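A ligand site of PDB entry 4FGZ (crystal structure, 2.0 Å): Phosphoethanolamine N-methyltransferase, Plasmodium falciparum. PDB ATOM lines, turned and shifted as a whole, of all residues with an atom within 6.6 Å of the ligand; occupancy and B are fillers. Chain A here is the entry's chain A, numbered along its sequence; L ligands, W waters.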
ATOM      1  N   GLU A  28      28.309 -15.080  -0.147  1.00  0.00           N
ATOM      2  CA  GLU A  28      27.266 -14.799   0.832  1.00  0.00           C
ATOM      3  C   GLU A  28      27.786 -14.858   2.255  1.00  0.00           C
ATOM      4  O   GLU A  28      27.335 -14.098   3.124  1.00  0.00           O
ATOM      5  CB  GLU A  28      26.134 -15.832   0.686  1.00  0.00           C
ATOM      6  CG  GLU A  28      24.847 -15.229   0.273  1.00  0.00           C
ATOM      7  CD  GLU A  28      23.677 -16.189   0.424  1.00  0.00           C
ATOM      8  OE1 GLU A  28      23.894 -17.422   0.564  1.00  0.00           O
ATOM      9  OE2 GLU A  28      22.530 -15.697   0.391  1.00  0.00           O
ATOM     10  N   PHE A  29      28.697 -15.785   2.529  1.00  0.00           N
ATOM     11  CA  PHE A  29      29.264 -15.921   3.865  1.00  0.00           C
ATOM     12  C   PHE A  29      29.940 -14.610   4.296  1.00  0.00           C
ATOM     13  O   PHE A  29      29.867 -14.210   5.457  1.00  0.00           O
ATOM     14  CB  PHE A  29      30.273 -17.071   3.923  1.00  0.00           C
ATOM     15  CG  PHE A  29      30.916 -17.266   5.273  1.00  0.00           C
ATOM     16  CD1 PHE A  29      32.045 -16.532   5.635  1.00  0.00           C
ATOM     17  CD2 PHE A  29      30.407 -18.190   6.172  1.00  0.00           C
ATOM     18  CE1 PHE A  29      32.637 -16.717   6.884  1.00  0.00           C
ATOM     19  CE2 PHE A  29      30.998 -18.376   7.422  1.00  0.00           C
ATOM     20  CZ  PHE A  29      32.110 -17.638   7.781  1.00  0.00           C
ATOM     21  N   ILE A  30      30.573 -13.958   3.336  1.00  0.00           N
ATOM     22  CA  ILE A  30      31.403 -12.801   3.646  1.00  0.00           C
ATOM     23  C   ILE A  30      30.658 -11.464   3.481  1.00  0.00           C
ATOM     24  O   ILE A  30      30.945 -10.513   4.217  1.00  0.00           O
ATOM     25  CB  ILE A  30      32.746 -12.847   2.846  1.00  0.00           C
ATOM     26  CG1 ILE A  30      33.831 -12.035   3.554  1.00  0.00           C
ATOM     27  CG2 ILE A  30      32.564 -12.427   1.398  1.00  0.00           C
ATOM     28  CD1 ILE A  30      35.191 -12.101   2.881  1.00  0.00           C
ATOM     29  N   PHE A  31      29.685 -11.411   2.574  1.00  0.00           N
ATOM     30  CA  PHE A  31      28.907 -10.180   2.355  1.00  0.00           C
ATOM     31  C   PHE A  31      27.629 -10.154   3.176  1.00  0.00           C
ATOM     32  O   PHE A  31      27.043  -9.081   3.424  1.00  0.00           O
ATOM     33  CB  PHE A  31      28.529 -10.012   0.877  1.00  0.00           C
ATOM     34  CG  PHE A  31      29.712  -9.838  -0.042  1.00  0.00           C
ATOM     35  CD1 PHE A  31      30.601  -8.786   0.133  1.00  0.00           C
ATOM     36  CD2 PHE A  31      29.913 -10.715  -1.108  1.00  0.00           C
ATOM     37  CE1 PHE A  31      31.687  -8.614  -0.721  1.00  0.00           C
ATOM     38  CE2 PHE A  31      31.008 -10.561  -1.975  1.00  0.00           C
ATOM     39  CZ  PHE A  31      31.902  -9.508  -1.783  1.00  0.00           C
ATOM     40  N   GLY A  32      27.172 -11.332   3.585  1.00  0.00           N
ATOM     41  CA  GLY A  32      25.895 -11.501   4.259  1.00  0.00           C
ATOM     42  C   GLY A  32      24.829 -12.095   3.360  1.00  0.00           C
ATOM     43  O   GLY A  32      24.944 -12.097   2.137  1.00  0.00           O
ATOM     44  N   GLU A  33      23.781 -12.616   3.992  1.00  0.00           N
ATOM     45  CA  GLU A  33      22.674 -13.290   3.308  1.00  0.00           C
ATOM     46  C   GLU A  33      22.095 -12.475   2.137  1.00  0.00           C
ATOM     47  O   GLU A  33      21.806 -11.288   2.283  1.00  0.00           O
ATOM     48  CB  GLU A  33      21.575 -13.604   4.325  1.00  0.00           C
ATOM     49  CG  GLU A  33      20.702 -14.780   3.943  1.00  0.00           C
ATOM     50  CD  GLU A  33      19.783 -15.223   5.083  1.00  0.00           C
ATOM     51  OE1 GLU A  33      19.413 -16.418   5.126  1.00  0.00           O
ATOM     52  OE2 GLU A  33      19.442 -14.364   5.939  1.00  0.00           O
ATOM     53  N   SER A  37      28.128  -8.967  -3.404  1.00  0.00           N
ATOM     54  CA  SER A  37      29.035  -7.869  -3.699  1.00  0.00           C
ATOM     55  C   SER A  37      29.301  -6.969  -2.480  1.00  0.00           C
ATOM     56  O   SER A  37      28.633  -7.084  -1.445  1.00  0.00           O
ATOM     57  CB  SER A  37      28.513  -7.045  -4.878  1.00  0.00           C
ATOM     58  OG  SER A  37      27.451  -6.191  -4.494  1.00  0.00           O
ATOM     59  N   SER A  38      30.292  -6.089  -2.656  1.00  0.00           N
ATOM     60  CA  SER A  38      30.855  -5.173  -1.659  1.00  0.00           C
ATOM     61  C   SER A  38      29.908  -4.656  -0.582  1.00  0.00           C
ATOM     62  O   SER A  38      28.951  -3.948  -0.889  1.00  0.00           O
ATOM     63  CB  SER A  38      31.470  -3.949  -2.376  1.00  0.00           C
ATOM     64  OG  SER A  38      32.263  -4.332  -3.474  1.00  0.00           O
ATOM     65  N   GLY A  39      30.186  -5.014   0.662  1.00  0.00           N
ATOM     66  CA  GLY A  39      29.513  -4.399   1.799  1.00  0.00           C
ATOM     67  C   GLY A  39      28.103  -4.917   2.092  1.00  0.00           C
ATOM     68  O   GLY A  39      27.474  -4.431   3.033  1.00  0.00           O
ATOM     69  N   GLY A  40      27.610  -5.865   1.299  1.00  0.00           N
ATOM     70  CA  GLY A  40      26.272  -6.437   1.481  1.00  0.00           C
ATOM     71  C   GLY A  40      25.188  -5.430   1.816  1.00  0.00           C
ATOM     72  O   GLY A  40      25.059  -4.380   1.168  1.00  0.00           O
ATOM     73  N   LEU A  41      24.410  -5.732   2.850  1.00  0.00           N
ATOM     74  CA  LEU A  41      23.262  -4.909   3.250  1.00  0.00           C
ATOM     75  C   LEU A  41      23.667  -3.507   3.718  1.00  0.00           C
ATOM     76  O   LEU A  41      23.035  -2.509   3.367  1.00  0.00           O
ATOM     77  CB  LEU A  41      22.494  -5.603   4.375  1.00  0.00           C
ATOM     78  CG  LEU A  41      21.328  -4.796   4.952  1.00  0.00           C
ATOM     79  CD1 LEU A  41      20.262  -4.543   3.869  1.00  0.00           C
ATOM     80  CD2 LEU A  41      20.730  -5.522   6.138  1.00  0.00           C
ATOM     81  N   GLU A  42      24.726  -3.444   4.505  1.00  0.00           N
ATOM     82  CA  GLU A  42      25.190  -2.163   5.059  1.00  0.00           C
ATOM     83  C   GLU A  42      25.546  -1.151   3.962  1.00  0.00           C
ATOM     84  O   GLU A  42      25.130   0.013   4.033  1.00  0.00           O
ATOM     85  CB  GLU A  42      26.353  -2.361   6.021  1.00  0.00           C
ATOM     86  CG  GLU A  42      26.001  -3.093   7.326  1.00  0.00           C
ATOM     87  CD  GLU A  42      26.015  -4.613   7.183  1.00  0.00           C
ATOM     88  OE1 GLU A  42      26.006  -5.119   6.023  1.00  0.00           O
ATOM     89  OE2 GLU A  42      26.051  -5.307   8.231  1.00  0.00           O
ATOM     90  N   ALA A  43      26.300  -1.584   2.952  1.00  0.00           N
ATOM     91  CA  ALA A  43      26.665  -0.659   1.874  1.00  0.00           C
ATOM     92  C   ALA A  43      25.434  -0.252   1.051  1.00  0.00           C
ATOM     93  O   ALA A  43      25.338   0.888   0.581  1.00  0.00           O
ATOM     94  CB  ALA A  43      27.758  -1.264   0.961  1.00  0.00           C
ATOM     95  N   LYS A  46      23.589   2.540   2.633  1.00  0.00           N
ATOM     96  CA  LYS A  46      24.294   3.788   2.298  1.00  0.00           C
ATOM     97  C   LYS A  46      24.038   4.253   0.854  1.00  0.00           C
ATOM     98  O   LYS A  46      23.712   5.412   0.613  1.00  0.00           O
ATOM     99  CB  LYS A  46      25.797   3.645   2.539  1.00  0.00           C
ATOM    100  CG  LYS A  46      26.619   4.875   2.134  1.00  0.00           C
ATOM    101  CD  LYS A  46      26.040   6.150   2.776  1.00  0.00           C
ATOM    102  CE  LYS A  46      27.123   7.009   3.441  1.00  0.00           C
ATOM    103  NZ  LYS A  46      26.572   8.320   3.908  1.00  0.00           N
ATOM    104  N   TYR A 209      36.271   4.196   0.976  1.00  0.00           N
ATOM    105  CA  TYR A 209      35.163   3.470   1.602  1.00  0.00           C
ATOM    106  C   TYR A 209      35.222   1.984   1.232  1.00  0.00           C
ATOM    107  O   TYR A 209      35.050   1.121   2.094  1.00  0.00           O
ATOM    108  CB  TYR A 209      33.837   4.128   1.219  1.00  0.00           C
ATOM    109  CG  TYR A 209      32.553   3.467   1.743  1.00  0.00           C
ATOM    110  CD1 TYR A 209      32.335   3.270   3.094  1.00  0.00           C
ATOM    111  CD2 TYR A 209      31.542   3.115   0.849  1.00  0.00           C
ATOM    112  CE1 TYR A 209      31.128   2.681   3.555  1.00  0.00           C
ATOM    113  CE2 TYR A 209      30.347   2.551   1.300  1.00  0.00           C
ATOM    114  CZ  TYR A 209      30.143   2.329   2.643  1.00  0.00           C
ATOM    115  OH  TYR A 209      28.948   1.767   3.039  1.00  0.00           O
ATOM    116  N   GLN A 212      37.600   0.184   3.338  1.00  0.00           N
ATOM    117  CA  GLN A 212      37.022  -0.083   4.655  1.00  0.00           C
ATOM    118  C   GLN A 212      36.100  -1.308   4.650  1.00  0.00           C
ATOM    119  O   GLN A 212      36.137  -2.130   5.573  1.00  0.00           O
ATOM    120  CB  GLN A 212      36.235   1.133   5.189  1.00  0.00           C
ATOM    121  CG  GLN A 212      37.128   2.343   5.511  1.00  0.00           C
ATOM    122  CD  GLN A 212      36.301   3.536   5.949  1.00  0.00           C
ATOM    123  OE1 GLN A 212      35.397   3.976   5.223  1.00  0.00           O
ATOM    124  NE2 GLN A 212      36.578   4.038   7.140  1.00  0.00           N
ATOM    125  N   LEU A 213      35.278  -1.439   3.601  1.00  0.00           N
ATOM    126  CA  LEU A 213      34.397  -2.610   3.494  1.00  0.00           C
ATOM    127  C   LEU A 213      35.212  -3.899   3.396  1.00  0.00           C
ATOM    128  O   LEU A 213      34.921  -4.891   4.084  1.00  0.00           O
ATOM    129  CB  LEU A 213      33.468  -2.494   2.270  1.00  0.00           C
ATOM    130  CG  LEU A 213      32.531  -1.296   2.193  1.00  0.00           C
ATOM    131  CD1 LEU A 213      31.830  -1.242   0.833  1.00  0.00           C
ATOM    132  CD2 LEU A 213      31.507  -1.298   3.376  1.00  0.00           C
ATOM    133  N   LEU A 214      36.238  -3.874   2.545  1.00  0.00           N
ATOM    134  CA  LEU A 214      37.085  -5.043   2.334  1.00  0.00           C
ATOM    135  C   LEU A 214      37.782  -5.445   3.614  1.00  0.00           C
ATOM    136  O   LEU A 214      37.932  -6.626   3.911  1.00  0.00           O
ATOM    137  CB  LEU A 214      38.134  -4.747   1.252  1.00  0.00           C
ATOM    138  CG  LEU A 214      37.727  -4.592  -0.207  1.00  0.00           C
ATOM    139  CD1 LEU A 214      38.896  -4.020  -1.020  1.00  0.00           C
ATOM    140  CD2 LEU A 214      37.272  -5.928  -0.791  1.00  0.00           C
ATOM    141  N   VAL A 216      36.686  -4.873   6.800  1.00  0.00           N
ATOM    142  CA  VAL A 216      35.698  -5.524   7.656  1.00  0.00           C
ATOM    143  C   VAL A 216      35.466  -6.976   7.201  1.00  0.00           C
ATOM    144  O   VAL A 216      35.492  -7.917   8.000  1.00  0.00           O
ATOM    145  CB  VAL A 216      34.367  -4.748   7.668  1.00  0.00           C
ATOM    146  CG1 VAL A 216      33.248  -5.597   8.278  1.00  0.00           C
ATOM    147  CG2 VAL A 216      34.534  -3.433   8.442  1.00  0.00           C
ATOM    148  N   GLU A 217      35.274  -7.158   5.899  1.00  0.00           N
ATOM    149  CA  GLU A 217      35.071  -8.496   5.343  1.00  0.00           C
ATOM    150  C   GLU A 217      36.238  -9.442   5.616  1.00  0.00           C
ATOM    151  O   GLU A 217      36.038 -10.597   6.009  1.00  0.00           O
ATOM    152  CB  GLU A 217      34.786  -8.409   3.833  1.00  0.00           C
ATOM    153  CG  GLU A 217      33.368  -7.969   3.541  1.00  0.00           C
ATOM    154  CD  GLU A 217      33.230  -7.103   2.303  1.00  0.00           C
ATOM    155  OE1 GLU A 217      34.194  -6.984   1.534  1.00  0.00           O
ATOM    156  OE2 GLU A 217      32.140  -6.516   2.104  1.00  0.00           O
ATOM    157  N   TYR A 220      36.393 -10.311   9.271  1.00  0.00           N
ATOM    158  CA  TYR A 220      35.271 -11.197   9.550  1.00  0.00           C
ATOM    159  C   TYR A 220      35.577 -12.631   9.136  1.00  0.00           C
ATOM    160  O   TYR A 220      35.229 -13.581   9.830  1.00  0.00           O
ATOM    161  CB  TYR A 220      34.019 -10.710   8.835  1.00  0.00           C
ATOM    162  CG  TYR A 220      32.780 -11.545   9.081  1.00  0.00           C
ATOM    163  CD1 TYR A 220      32.456 -12.620   8.253  1.00  0.00           C
ATOM    164  CD2 TYR A 220      31.921 -11.253  10.134  1.00  0.00           C
ATOM    165  CE1 TYR A 220      31.337 -13.374   8.472  1.00  0.00           C
ATOM    166  CE2 TYR A 220      30.779 -12.002  10.359  1.00  0.00           C
ATOM    167  CZ  TYR A 220      30.494 -13.056   9.532  1.00  0.00           C
ATOM    168  OH  TYR A 220      29.372 -13.803   9.746  1.00  0.00           O
HETATM  169  C1  LIG L   1      30.747   1.317  10.381  1.00  0.00           C
HETATM  170  C2  LIG L   1      31.012  -0.053  10.723  1.00  0.00           C
HETATM  171  C3  LIG L   1      30.778  -1.063   9.793  1.00  0.00           C
HETATM  172  C4  LIG L   1      30.249  -0.712   8.510  1.00  0.00           C
HETATM  173  C5  LIG L   1      29.978   0.608   8.176  1.00  0.00           C
HETATM  174  C6  LIG L   1      30.232   1.637   9.119  1.00  0.00           C
HETATM  175  C7  LIG L   1      30.006  -1.732   7.534  1.00  0.00           C
HETATM  176  C8  LIG L   1      29.492  -1.363   6.246  1.00  0.00           C
HETATM  177  C9  LIG L   1      29.240  -0.013   5.961  1.00  0.00           C
HETATM  178  N1  LIG L   1      29.469   0.927   6.907  1.00  0.00           N
HETATM  179 CL1  LIG L   1      31.067   2.550  11.566  1.00  0.00          CL
HETATM  180  N2  LIG L   1      30.300  -3.127   7.894  1.00  0.00           N
HETATM  181  C10 LIG L   1      30.329  -4.160   6.859  1.00  0.00           C
HETATM  182  C11 LIG L   1      31.291  -4.059   5.825  1.00  0.00           C
HETATM  183  C12 LIG L   1      31.331  -5.047   4.827  1.00  0.00           C
HETATM  184  C13 LIG L   1      30.415  -6.122   4.879  1.00  0.00           C
HETATM  185  C14 LIG L   1      29.463  -6.234   5.912  1.00  0.00           C
HETATM  186  C15 LIG L   1      29.431  -5.231   6.925  1.00  0.00           C
HETATM  187  O1  LIG L   1      30.439  -7.120   3.897  1.00  0.00           O
HETATM  188  C16 LIG L   1      28.498  -7.434   5.916  1.00  0.00           C
HETATM  189  N3  LIG L   1      28.889  -8.611   6.743  1.00  0.00           N
HETATM  190  C17 LIG L   1      30.318  -8.880   6.782  1.00  0.00           C
HETATM  191  C18 LIG L   1      31.014  -8.569   8.063  1.00  0.00           C
HETATM  192  C19 LIG L   1      28.088  -9.831   6.530  1.00  0.00           C
HETATM  193  C20 LIG L   1      28.696 -11.167   6.848  1.00  0.00           C
HETATM  194  O   HOH W   1      28.054   2.926   5.439  1.00  0.00           O
HETATM  195  O   HOH W   2      30.342  -4.574  10.548  1.00  0.00           O
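OE2 of Glu 217 is in hydrogen-bond range of N of Gly 39, at 2.9 Å.
OE2 of Glu 217 is in hydrogen-bond range of O1 of the ligand. O of Ile 30 sits close to O1 of the ligand (3.4 Å).
Water W1 lies within hydrogen-bond range of OH of Tyr 209 (2.8 Å) and N1 of the ligand (2.9 Å).
O of Phe 29 touches C20 of the ligand (3.5 Å). O of Phe 31 touches C16 of the ligand, 3.3 Å away. N of Gly 32 touches C19 of the ligand, at 3.4 Å. Gly 39 touches the ligand. Glu 42 touches the ligand. OH of Tyr 209 touches C9 of the ligand, 3.4 Å away. Leu 213 touches the ligand (CD2 to C8, 3.5 Å). Val 216 touches the ligand (CG1 to C11, 3.5 Å). Tyr 220 touches the ligand. Hydrophobic or aromatic side chains that line the ligand: Leu 213, Val 216 and Tyr 220. Within 4 Å of the ligand: Phe 29, Ile 30, Phe 31, Gly 32, Gly 39, Glu 42, Tyr 209, Leu 213, Val 216, Glu 217 and Tyr 220.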
